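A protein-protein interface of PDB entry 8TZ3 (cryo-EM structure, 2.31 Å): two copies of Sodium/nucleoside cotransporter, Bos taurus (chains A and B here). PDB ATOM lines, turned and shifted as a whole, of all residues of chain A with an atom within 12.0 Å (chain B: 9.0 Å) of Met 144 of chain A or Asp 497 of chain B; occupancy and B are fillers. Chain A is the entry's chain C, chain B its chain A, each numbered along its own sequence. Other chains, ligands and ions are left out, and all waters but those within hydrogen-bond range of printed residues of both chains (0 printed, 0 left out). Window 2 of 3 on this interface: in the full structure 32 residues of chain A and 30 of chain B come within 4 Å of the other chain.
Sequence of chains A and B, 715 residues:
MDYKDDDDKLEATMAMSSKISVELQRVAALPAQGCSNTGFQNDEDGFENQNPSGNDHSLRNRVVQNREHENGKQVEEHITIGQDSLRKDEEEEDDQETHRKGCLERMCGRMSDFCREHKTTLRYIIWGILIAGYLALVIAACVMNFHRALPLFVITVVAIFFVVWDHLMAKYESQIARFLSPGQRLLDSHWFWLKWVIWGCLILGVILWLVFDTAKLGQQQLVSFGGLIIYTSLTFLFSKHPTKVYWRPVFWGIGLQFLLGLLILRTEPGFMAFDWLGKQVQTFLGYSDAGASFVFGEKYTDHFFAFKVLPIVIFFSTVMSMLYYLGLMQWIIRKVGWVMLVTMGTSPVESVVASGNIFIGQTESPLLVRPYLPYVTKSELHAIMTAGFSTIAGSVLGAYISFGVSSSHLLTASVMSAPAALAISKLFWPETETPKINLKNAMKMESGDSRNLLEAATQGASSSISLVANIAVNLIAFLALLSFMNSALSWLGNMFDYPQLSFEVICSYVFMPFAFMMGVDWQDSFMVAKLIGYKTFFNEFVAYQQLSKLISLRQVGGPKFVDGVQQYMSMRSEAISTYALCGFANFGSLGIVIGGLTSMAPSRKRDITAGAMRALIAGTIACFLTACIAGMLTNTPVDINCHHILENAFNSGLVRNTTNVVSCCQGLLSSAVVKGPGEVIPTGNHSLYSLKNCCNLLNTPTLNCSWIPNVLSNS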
ATOM      1  N   LEU A 135       2.297  18.887 -17.115  1.00  0.00           N
ATOM      2  CA  LEU A 135       1.311  19.873 -17.545  1.00  0.00           C
ATOM      3  C   LEU A 135      -0.092  19.491 -17.097  1.00  0.00           C
ATOM      4  O   LEU A 135      -0.904  20.364 -16.770  1.00  0.00           O
ATOM      5  CB  LEU A 135       1.354  20.040 -19.063  1.00  0.00           C
ATOM      6  CG  LEU A 135       2.661  20.559 -19.662  1.00  0.00           C
ATOM      7  CD1 LEU A 135       2.561  20.640 -21.175  1.00  0.00           C
ATOM      8  CD2 LEU A 135       3.021  21.912 -19.083  1.00  0.00           C
ATOM      9  N   ALA A 136      -0.401  18.193 -17.079  1.00  0.00           N
ATOM     10  CA  ALA A 136      -1.723  17.764 -16.638  1.00  0.00           C
ATOM     11  C   ALA A 136      -1.934  18.078 -15.163  1.00  0.00           C
ATOM     12  O   ALA A 136      -3.011  18.535 -14.763  1.00  0.00           O
ATOM     13  CB  ALA A 136      -1.902  16.270 -16.899  1.00  0.00           C
ATOM     14  N   LEU A 137      -0.915  17.837 -14.338  1.00  0.00           N
ATOM     15  CA  LEU A 137      -1.015  18.176 -12.924  1.00  0.00           C
ATOM     16  C   LEU A 137      -1.210  19.673 -12.732  1.00  0.00           C
ATOM     17  O   LEU A 137      -2.027  20.102 -11.910  1.00  0.00           O
ATOM     18  CB  LEU A 137       0.235  17.698 -12.188  1.00  0.00           C
ATOM     19  CG  LEU A 137       0.492  16.193 -12.145  1.00  0.00           C
ATOM     20  CD1 LEU A 137       1.798  15.932 -11.413  1.00  0.00           C
ATOM     21  CD2 LEU A 137      -0.657  15.444 -11.481  1.00  0.00           C
ATOM     22  N   VAL A 138      -0.477  20.485 -13.493  1.00  0.00           N
ATOM     23  CA  VAL A 138      -0.580  21.935 -13.353  1.00  0.00           C
ATOM     24  C   VAL A 138      -1.975  22.407 -13.737  1.00  0.00           C
ATOM     25  O   VAL A 138      -2.639  23.124 -12.979  1.00  0.00           O
ATOM     26  CB  VAL A 138       0.502  22.633 -14.196  1.00  0.00           C
ATOM     27  CG1 VAL A 138       0.365  24.136 -14.085  1.00  0.00           C
ATOM     28  CG2 VAL A 138       1.883  22.194 -13.761  1.00  0.00           C
ATOM     29  N   ILE A 139      -2.439  22.021 -14.926  1.00  0.00           N
ATOM     30  CA  ILE A 139      -3.743  22.481 -15.390  1.00  0.00           C
ATOM     31  C   ILE A 139      -4.840  22.013 -14.442  1.00  0.00           C
ATOM     32  O   ILE A 139      -5.759  22.772 -14.110  1.00  0.00           O
ATOM     33  CB  ILE A 139      -3.997  22.013 -16.835  1.00  0.00           C
ATOM     34  CG1 ILE A 139      -5.304  22.608 -17.352  1.00  0.00           C
ATOM     35  CG2 ILE A 139      -4.040  20.496 -16.914  1.00  0.00           C
ATOM     36  CD1 ILE A 139      -5.548  22.371 -18.821  1.00  0.00           C
ATOM     37  N   ALA A 140      -4.760  20.763 -13.986  1.00  0.00           N
ATOM     38  CA  ALA A 140      -5.734  20.268 -13.022  1.00  0.00           C
ATOM     39  C   ALA A 140      -5.713  21.091 -11.742  1.00  0.00           C
ATOM     40  O   ALA A 140      -6.769  21.430 -11.195  1.00  0.00           O
ATOM     41  CB  ALA A 140      -5.464  18.797 -12.717  1.00  0.00           C
ATOM     42  N   ALA A 141      -4.521  21.415 -11.243  1.00  0.00           N
ATOM     43  CA  ALA A 141      -4.419  22.225 -10.033  1.00  0.00           C
ATOM     44  C   ALA A 141      -5.130  23.560 -10.201  1.00  0.00           C
ATOM     45  O   ALA A 141      -5.933  23.961  -9.351  1.00  0.00           O
ATOM     46  CB  ALA A 141      -2.954  22.445  -9.676  1.00  0.00           C
ATOM     47  N   CYS A 142      -4.843  24.270 -11.294  1.00  0.00           N
ATOM     48  CA  CYS A 142      -5.466  25.572 -11.500  1.00  0.00           C
ATOM     49  C   CYS A 142      -6.980  25.445 -11.608  1.00  0.00           C
ATOM     50  O   CYS A 142      -7.720  26.317 -11.141  1.00  0.00           O
ATOM     51  CB  CYS A 142      -4.896  26.238 -12.752  1.00  0.00           C
ATOM     52  SG  CYS A 142      -3.138  26.654 -12.668  1.00  0.00           S
ATOM     53  N   VAL A 143      -7.458  24.361 -12.220  1.00  0.00           N
ATOM     54  CA  VAL A 143      -8.897  24.147 -12.343  1.00  0.00           C
ATOM     55  C   VAL A 143      -9.533  24.014 -10.964  1.00  0.00           C
ATOM     56  O   VAL A 143     -10.527  24.678 -10.652  1.00  0.00           O
ATOM     57  CB  VAL A 143      -9.176  22.917 -13.224  1.00  0.00           C
ATOM     58  CG1 VAL A 143     -10.607  22.449 -13.062  1.00  0.00           C
ATOM     59  CG2 VAL A 143      -8.886  23.240 -14.678  1.00  0.00           C
ATOM     60  N   MET A 144      -8.966  23.153 -10.116  1.00  0.00           N
ATOM     61  CA  MET A 144      -9.505  22.979  -8.771  1.00  0.00           C
ATOM     62  C   MET A 144      -9.482  24.287  -7.988  1.00  0.00           C
ATOM     63  O   MET A 144     -10.408  24.575  -7.222  1.00  0.00           O
ATOM     64  CB  MET A 144      -8.721  21.897  -8.029  1.00  0.00           C
ATOM     65  CG  MET A 144      -8.740  20.542  -8.718  1.00  0.00           C
ATOM     66  SD  MET A 144      -7.959  19.229  -7.764  1.00  0.00           S
ATOM     67  CE  MET A 144      -9.022  19.195  -6.325  1.00  0.00           C
ATOM     68  N   ASN A 145      -8.430  25.086  -8.159  1.00  0.00           N
ATOM     69  CA  ASN A 145      -8.315  26.370  -7.478  1.00  0.00           C
ATOM     70  C   ASN A 145      -7.100  27.127  -7.996  1.00  0.00           C
ATOM     71  O   ASN A 145      -5.962  26.683  -7.817  1.00  0.00           O
ATOM     72  CB  ASN A 145      -8.221  26.173  -5.966  1.00  0.00           C
ATOM     73  CG  ASN A 145      -8.154  27.482  -5.205  1.00  0.00           C
ATOM     74  OD1 ASN A 145      -7.840  28.531  -5.766  1.00  0.00           O
ATOM     75  ND2 ASN A 145      -8.443  27.423  -3.914  1.00  0.00           N
ATOM     76  N   PHE A 146      -7.333  28.282  -8.619  1.00  0.00           N
ATOM     77  CA  PHE A 146      -6.290  29.023  -9.317  1.00  0.00           C
ATOM     78  C   PHE A 146      -5.400  29.817  -8.365  1.00  0.00           C
ATOM     79  O   PHE A 146      -4.172  29.779  -8.485  1.00  0.00           O
ATOM     80  CB  PHE A 146      -6.922  29.963 -10.345  1.00  0.00           C
ATOM     81  CG  PHE A 146      -5.949  30.507 -11.341  1.00  0.00           C
ATOM     82  CD1 PHE A 146      -5.706  29.836 -12.523  1.00  0.00           C
ATOM     83  CD2 PHE A 146      -5.273  31.685 -11.096  1.00  0.00           C
ATOM     84  CE1 PHE A 146      -4.807  30.331 -13.445  1.00  0.00           C
ATOM     85  CE2 PHE A 146      -4.373  32.185 -12.012  1.00  0.00           C
ATOM     86  CZ  PHE A 146      -4.139  31.506 -13.189  1.00  0.00           C
ATOM     87  N   HIS A 147      -6.002  30.544  -7.421  1.00  0.00           N
ATOM     88  CA  HIS A 147      -5.212  31.382  -6.526  1.00  0.00           C
ATOM     89  C   HIS A 147      -4.224  30.554  -5.716  1.00  0.00           C
ATOM     90  O   HIS A 147      -3.101  31.000  -5.454  1.00  0.00           O
ATOM     91  CB  HIS A 147      -6.137  32.166  -5.597  1.00  0.00           C
ATOM     92  CG  HIS A 147      -5.417  33.048  -4.625  1.00  0.00           C
ATOM     93  ND1 HIS A 147      -4.663  34.131  -5.019  1.00  0.00           N
ATOM     94  CD2 HIS A 147      -5.343  33.010  -3.273  1.00  0.00           C
ATOM     95  CE1 HIS A 147      -4.152  34.722  -3.954  1.00  0.00           C
ATOM     96  NE2 HIS A 147      -4.549  34.061  -2.881  1.00  0.00           N
ATOM     97  N   ARG A 148      -4.627  29.352  -5.309  1.00  0.00           N
ATOM     98  CA  ARG A 148      -3.734  28.478  -4.562  1.00  0.00           C
ATOM     99  C   ARG A 148      -2.616  27.932  -5.440  1.00  0.00           C
ATOM    100  O   ARG A 148      -1.511  27.688  -4.948  1.00  0.00           O
ATOM    101  CB  ARG A 148      -4.540  27.336  -3.948  1.00  0.00           C
ATOM    102  CG  ARG A 148      -3.775  26.461  -2.977  1.00  0.00           C
ATOM    103  CD  ARG A 148      -4.691  25.444  -2.336  1.00  0.00           C
ATOM    104  NE  ARG A 148      -5.443  24.688  -3.326  1.00  0.00           N
ATOM    105  CZ  ARG A 148      -6.461  23.888  -3.043  1.00  0.00           C
ATOM    106  NH1 ARG A 148      -6.887  23.727  -1.803  1.00  0.00           N
ATOM    107  NH2 ARG A 148      -7.065  23.237  -4.028  1.00  0.00           N
ATOM    108  N   ALA A 149      -2.878  27.745  -6.731  1.00  0.00           N
ATOM    109  CA  ALA A 149      -1.925  27.155  -7.655  1.00  0.00           C
ATOM    110  C   ALA A 149      -1.124  28.189  -8.433  1.00  0.00           C
ATOM    111  O   ALA A 149      -0.374  27.819  -9.341  1.00  0.00           O
ATOM    112  CB  ALA A 149      -2.652  26.236  -8.634  1.00  0.00           C
ATOM    113  N   LEU A 150      -1.260  29.468  -8.101  1.00  0.00           N
ATOM    114  CA  LEU A 150      -0.609  30.509  -8.892  1.00  0.00           C
ATOM    115  C   LEU A 150       0.901  30.345  -8.951  1.00  0.00           C
ATOM    116  O   LEU A 150       1.465  30.418 -10.057  1.00  0.00           O
ATOM    117  CB  LEU A 150      -0.994  31.881  -8.334  1.00  0.00           C
ATOM    118  CG  LEU A 150      -0.620  33.086  -9.193  1.00  0.00           C
ATOM    119  CD1 LEU A 150      -1.447  33.114 -10.469  1.00  0.00           C
ATOM    120  CD2 LEU A 150      -0.796  34.361  -8.407  1.00  0.00           C
ATOM    121  N   LEU A 152       2.735  27.811  -8.943  1.00  0.00           N
ATOM    122  CA  LEU A 152       3.127  26.707  -9.809  1.00  0.00           C
ATOM    123  C   LEU A 152       2.829  27.023 -11.268  1.00  0.00           C
ATOM    124  O   LEU A 152       3.469  26.476 -12.173  1.00  0.00           O
ATOM    125  CB  LEU A 152       2.418  25.429  -9.373  1.00  0.00           C
ATOM    126  CG  LEU A 152       2.669  24.170 -10.197  1.00  0.00           C
ATOM    127  CD1 LEU A 152       4.075  23.641  -9.985  1.00  0.00           C
ATOM    128  CD2 LEU A 152       1.638  23.133  -9.845  1.00  0.00           C
ATOM    129  N   PHE A 153       1.856  27.898 -11.515  1.00  0.00           N
ATOM    130  CA  PHE A 153       1.587  28.341 -12.877  1.00  0.00           C
ATOM    131  C   PHE A 153       2.643  29.329 -13.353  1.00  0.00           C
ATOM    132  O   PHE A 153       3.080  29.276 -14.507  1.00  0.00           O
ATOM    133  CB  PHE A 153       0.193  28.959 -12.945  1.00  0.00           C
ATOM    134  CG  PHE A 153      -0.178  29.476 -14.298  1.00  0.00           C
ATOM    135  CD1 PHE A 153      -0.481  28.603 -15.326  1.00  0.00           C
ATOM    136  CD2 PHE A 153      -0.234  30.835 -14.543  1.00  0.00           C
ATOM    137  CE1 PHE A 153      -0.823  29.076 -16.571  1.00  0.00           C
ATOM    138  CE2 PHE A 153      -0.575  31.312 -15.785  1.00  0.00           C
ATOM    139  CZ  PHE A 153      -0.873  30.434 -16.801  1.00  0.00           C
ATOM    140  N   SER B 490       4.218  18.518  -0.097  1.00  0.00           N
ATOM    141  CA  SER B 490       3.001  18.962   0.565  1.00  0.00           C
ATOM    142  C   SER B 490       2.488  20.259  -0.044  1.00  0.00           C
ATOM    143  O   SER B 490       1.276  20.441  -0.206  1.00  0.00           O
ATOM    144  CB  SER B 490       3.267  19.134   2.055  1.00  0.00           C
ATOM    145  OG  SER B 490       2.072  19.282   2.788  1.00  0.00           O
ATOM    146  N   TRP B 491       3.398  21.177  -0.366  1.00  0.00           N
ATOM    147  CA  TRP B 491       3.036  22.372  -1.113  1.00  0.00           C
ATOM    148  C   TRP B 491       2.314  22.017  -2.405  1.00  0.00           C
ATOM    149  O   TRP B 491       1.278  22.605  -2.730  1.00  0.00           O
ATOM    150  CB  TRP B 491       4.305  23.178  -1.386  1.00  0.00           C
ATOM    151  CG  TRP B 491       4.141  24.419  -2.185  1.00  0.00           C
ATOM    152  CD1 TRP B 491       3.642  25.608  -1.759  1.00  0.00           C
ATOM    153  CD2 TRP B 491       4.511  24.608  -3.553  1.00  0.00           C
ATOM    154  NE1 TRP B 491       3.664  26.522  -2.774  1.00  0.00           N
ATOM    155  CE2 TRP B 491       4.194  25.934  -3.889  1.00  0.00           C
ATOM    156  CE3 TRP B 491       5.073  23.784  -4.527  1.00  0.00           C
ATOM    157  CZ2 TRP B 491       4.419  26.452  -5.156  1.00  0.00           C
ATOM    158  CZ3 TRP B 491       5.293  24.301  -5.779  1.00  0.00           C
ATOM    159  CH2 TRP B 491       4.969  25.621  -6.084  1.00  0.00           C
ATOM    160  N   LEU B 492       2.845  21.053  -3.153  1.00  0.00           N
ATOM    161  CA  LEU B 492       2.207  20.628  -4.392  1.00  0.00           C
ATOM    162  C   LEU B 492       0.902  19.883  -4.131  1.00  0.00           C
ATOM    163  O   LEU B 492      -0.112  20.162  -4.778  1.00  0.00           O
ATOM    164  CB  LEU B 492       3.170  19.760  -5.194  1.00  0.00           C
ATOM    165  CG  LEU B 492       2.612  19.040  -6.418  1.00  0.00           C
ATOM    166  CD1 LEU B 492       2.131  20.040  -7.439  1.00  0.00           C
ATOM    167  CD2 LEU B 492       3.661  18.127  -7.012  1.00  0.00           C
ATOM    168  N   GLY B 493       0.907  18.925  -3.205  1.00  0.00           N
ATOM    169  CA  GLY B 493      -0.304  18.181  -2.916  1.00  0.00           C
ATOM    170  C   GLY B 493      -1.463  19.053  -2.482  1.00  0.00           C
ATOM    171  O   GLY B 493      -2.600  18.832  -2.902  1.00  0.00           O
ATOM    172  N   ASN B 494      -1.199  20.040  -1.629  1.00  0.00           N
ATOM    173  CA  ASN B 494      -2.237  20.959  -1.184  1.00  0.00           C
ATOM    174  C   ASN B 494      -2.983  21.612  -2.342  1.00  0.00           C
ATOM    175  O   ASN B 494      -4.106  22.085  -2.149  1.00  0.00           O
ATOM    176  CB  ASN B 494      -1.617  22.026  -0.293  1.00  0.00           C
ATOM    177  CG  ASN B 494      -2.645  22.826   0.457  1.00  0.00           C
ATOM    178  OD1 ASN B 494      -3.551  22.274   1.076  1.00  0.00           O
ATOM    179  ND2 ASN B 494      -2.516  24.138   0.399  1.00  0.00           N
ATOM    180  N   MET B 495      -2.390  21.649  -3.535  1.00  0.00           N
ATOM    181  CA  MET B 495      -3.078  22.166  -4.708  1.00  0.00           C
ATOM    182  C   MET B 495      -4.134  21.212  -5.241  1.00  0.00           C
ATOM    183  O   MET B 495      -4.832  21.560  -6.197  1.00  0.00           O
ATOM    184  CB  MET B 495      -2.072  22.467  -5.812  1.00  0.00           C
ATOM    185  CG  MET B 495      -1.087  23.541  -5.454  1.00  0.00           C
ATOM    186  SD  MET B 495       0.115  23.868  -6.740  1.00  0.00           S
ATOM    187  CE  MET B 495       0.967  25.235  -5.983  1.00  0.00           C
ATOM    188  N   PHE B 496      -4.257  20.021  -4.659  1.00  0.00           N
ATOM    189  CA  PHE B 496      -5.300  19.071  -5.019  1.00  0.00           C
ATOM    190  C   PHE B 496      -6.058  18.596  -3.791  1.00  0.00           C
ATOM    191  O   PHE B 496      -6.755  17.581  -3.850  1.00  0.00           O
ATOM    192  CB  PHE B 496      -4.715  17.869  -5.756  1.00  0.00           C
ATOM    193  CG  PHE B 496      -3.788  18.226  -6.868  1.00  0.00           C
ATOM    194  CD1 PHE B 496      -2.434  18.344  -6.640  1.00  0.00           C
ATOM    195  CD2 PHE B 496      -4.263  18.423  -8.145  1.00  0.00           C
ATOM    196  CE1 PHE B 496      -1.580  18.663  -7.659  1.00  0.00           C
ATOM    197  CE2 PHE B 496      -3.410  18.742  -9.167  1.00  0.00           C
ATOM    198  CZ  PHE B 496      -2.066  18.863  -8.925  1.00  0.00           C
ATOM    199  N   ASP B 497      -5.916  19.306  -2.675  1.00  0.00           N
ATOM    200  CA  ASP B 497      -6.536  18.933  -1.410  1.00  0.00           C
ATOM    201  C   ASP B 497      -5.941  17.641  -0.858  1.00  0.00           C
ATOM    202  O   ASP B 497      -6.648  16.816  -0.276  1.00  0.00           O
ATOM    203  CB  ASP B 497      -8.055  18.815  -1.553  1.00  0.00           C
ATOM    204  CG  ASP B 497      -8.691  20.102  -2.033  1.00  0.00           C
ATOM    205  OD1 ASP B 497      -8.150  21.182  -1.720  1.00  0.00           O
ATOM    206  OD2 ASP B 497      -9.727  20.036  -2.724  1.00  0.00           O
ATOM    207  N   TYR B 498      -4.633  17.459  -1.038  1.00  0.00           N
ATOM    208  CA  TYR B 498      -3.908  16.292  -0.537  1.00  0.00           C
ATOM    209  C   TYR B 498      -2.550  16.729   0.000  1.00  0.00           C
ATOM    210  O   TYR B 498      -1.501  16.381  -0.552  1.00  0.00           O
ATOM    211  CB  TYR B 498      -3.753  15.230  -1.624  1.00  0.00           C
ATOM    212  CG  TYR B 498      -3.266  13.913  -1.090  1.00  0.00           C
ATOM    213  CD1 TYR B 498      -3.979  13.244  -0.115  1.00  0.00           C
ATOM    214  CD2 TYR B 498      -2.099  13.337  -1.553  1.00  0.00           C
ATOM    215  CE1 TYR B 498      -3.544  12.047   0.387  1.00  0.00           C
ATOM    216  CE2 TYR B 498      -1.658  12.139  -1.058  1.00  0.00           C
ATOM    217  CZ  TYR B 498      -2.383  11.497  -0.088  1.00  0.00           C
ATOM    218  OH  TYR B 498      -1.948  10.294   0.413  1.00  0.00           O
ATOM    219  N   PRO B 499      -2.538  17.493   1.094  1.00  0.00           N
ATOM    220  CA  PRO B 499      -1.271  17.953   1.676  1.00  0.00           C
ATOM    221  C   PRO B 499      -0.482  16.873   2.393  1.00  0.00           C
ATOM    222  O   PRO B 499       0.604  17.164   2.903  1.00  0.00           O
ATOM    223  CB  PRO B 499      -1.721  19.042   2.658  1.00  0.00           C
ATOM    224  CG  PRO B 499      -3.127  18.740   2.953  1.00  0.00           C
ATOM    225  CD  PRO B 499      -3.706  18.065   1.772  1.00  0.00           C
ATOM    226  N   GLN B 500      -0.990  15.647   2.449  1.00  0.00           N
ATOM    227  CA  GLN B 500      -0.287  14.539   3.070  1.00  0.00           C
ATOM    228  C   GLN B 500       0.787  13.945   2.175  1.00  0.00           C
ATOM    229  O   GLN B 500       1.602  13.152   2.656  1.00  0.00           O
ATOM    230  CB  GLN B 500      -1.285  13.449   3.455  1.00  0.00           C
ATOM    231  CG  GLN B 500      -2.354  13.898   4.412  1.00  0.00           C
ATOM    232  CD  GLN B 500      -3.543  14.514   3.711  1.00  0.00           C
ATOM    233  OE1 GLN B 500      -3.860  14.162   2.578  1.00  0.00           O
ATOM    234  NE2 GLN B 500      -4.211  15.437   4.385  1.00  0.00           N
ATOM    235  N   LEU B 501       0.793  14.299   0.894  1.00  0.00           N
ATOM    236  CA  LEU B 501       1.780  13.789  -0.042  1.00  0.00           C
ATOM    237  C   LEU B 501       3.186  13.897   0.533  1.00  0.00           C
ATOM    238  O   LEU B 501       3.575  14.938   1.068  1.00  0.00           O
ATOM    239  CB  LEU B 501       1.685  14.562  -1.350  1.00  0.00           C
ATOM    240  CG  LEU B 501       2.462  14.037  -2.553  1.00  0.00           C
ATOM    241  CD1 LEU B 501       1.922  12.714  -2.998  1.00  0.00           C
ATOM    242  CD2 LEU B 501       2.414  15.032  -3.682  1.00  0.00           C
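The backbone carbonyl oxygen (O) of Asn 494 of chain B sits close to the guanidinium group (NE) of Arg 148 of chain A, at 3.2 Å.
NH1 of Arg 148 of chain A lies within salt-bridge range of OD1 of Asp 497 of chain B, at 2.8 Å.
The side-chain amide oxygen (OD1) of Asn 145 of chain A lies within hydrogen-bond range of the backbone NH (N) of Arg 148 of chain A (3.3 Å).
CZ of Phe 496 of chain B touches O of Leu 137 of chain A (3.2 Å).
O of Met 495 of chain B touches CA of Ala 141 of chain A (3.9 Å).
Ala 141 of chain A touches Phe 496 of chain B (N to CE2, 3.6 Å).
CE of Met 144 of chain A touches O of Phe 496 of chain B, at 3.7 Å.
Asp 497 of chain B touches Met 144 of chain A.
Arg 148 of chain A touches Met 495 of chain B (NH2 to O, 3.5 Å).
CE of Met 495 of chain B touches CA of Ala 149 of chain A, at 3.9 Å.
CD2 of Leu 152 of chain A touches CD1 of Leu 492 of chain B (3.9 Å).
Met 495 of chain B touches Leu 152 of chain A.
Printed residues of chain B within 4 Å of Leu 137 of chain A: Phe 496.
No residue of chain B comes within 4 Å of Val 143 of chain A.
Met 144 of chain A touches just these residues of chain B: Phe 496 (3.7 Å) and Asp 497 (3.8 Å).
Asn 145 of chain A touches none of the printed residues of chain B.
Printed residues of chain B within 4 Å of Ala 149 of chain A: Met 495 (3.9 Å).
Of the printed residues of chain B, Leu 152 of chain A touches Leu 492 and Met 495.
Printed residues of chain A within 4 Å of Met 495 of chain B: Ala 141, Arg 148, Ala 149 and Leu 152.
Pro 499 of chain B touches none of the printed residues of chain A.
Printed residues of chain B that touch a printed residue of chain A: Leu 492, Asn 494, Met 495, Phe 496 and Asp 497.
Of the 18 printed residues of chain A, 6 touch a printed residue of chain B.
No position is printed for both chains.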
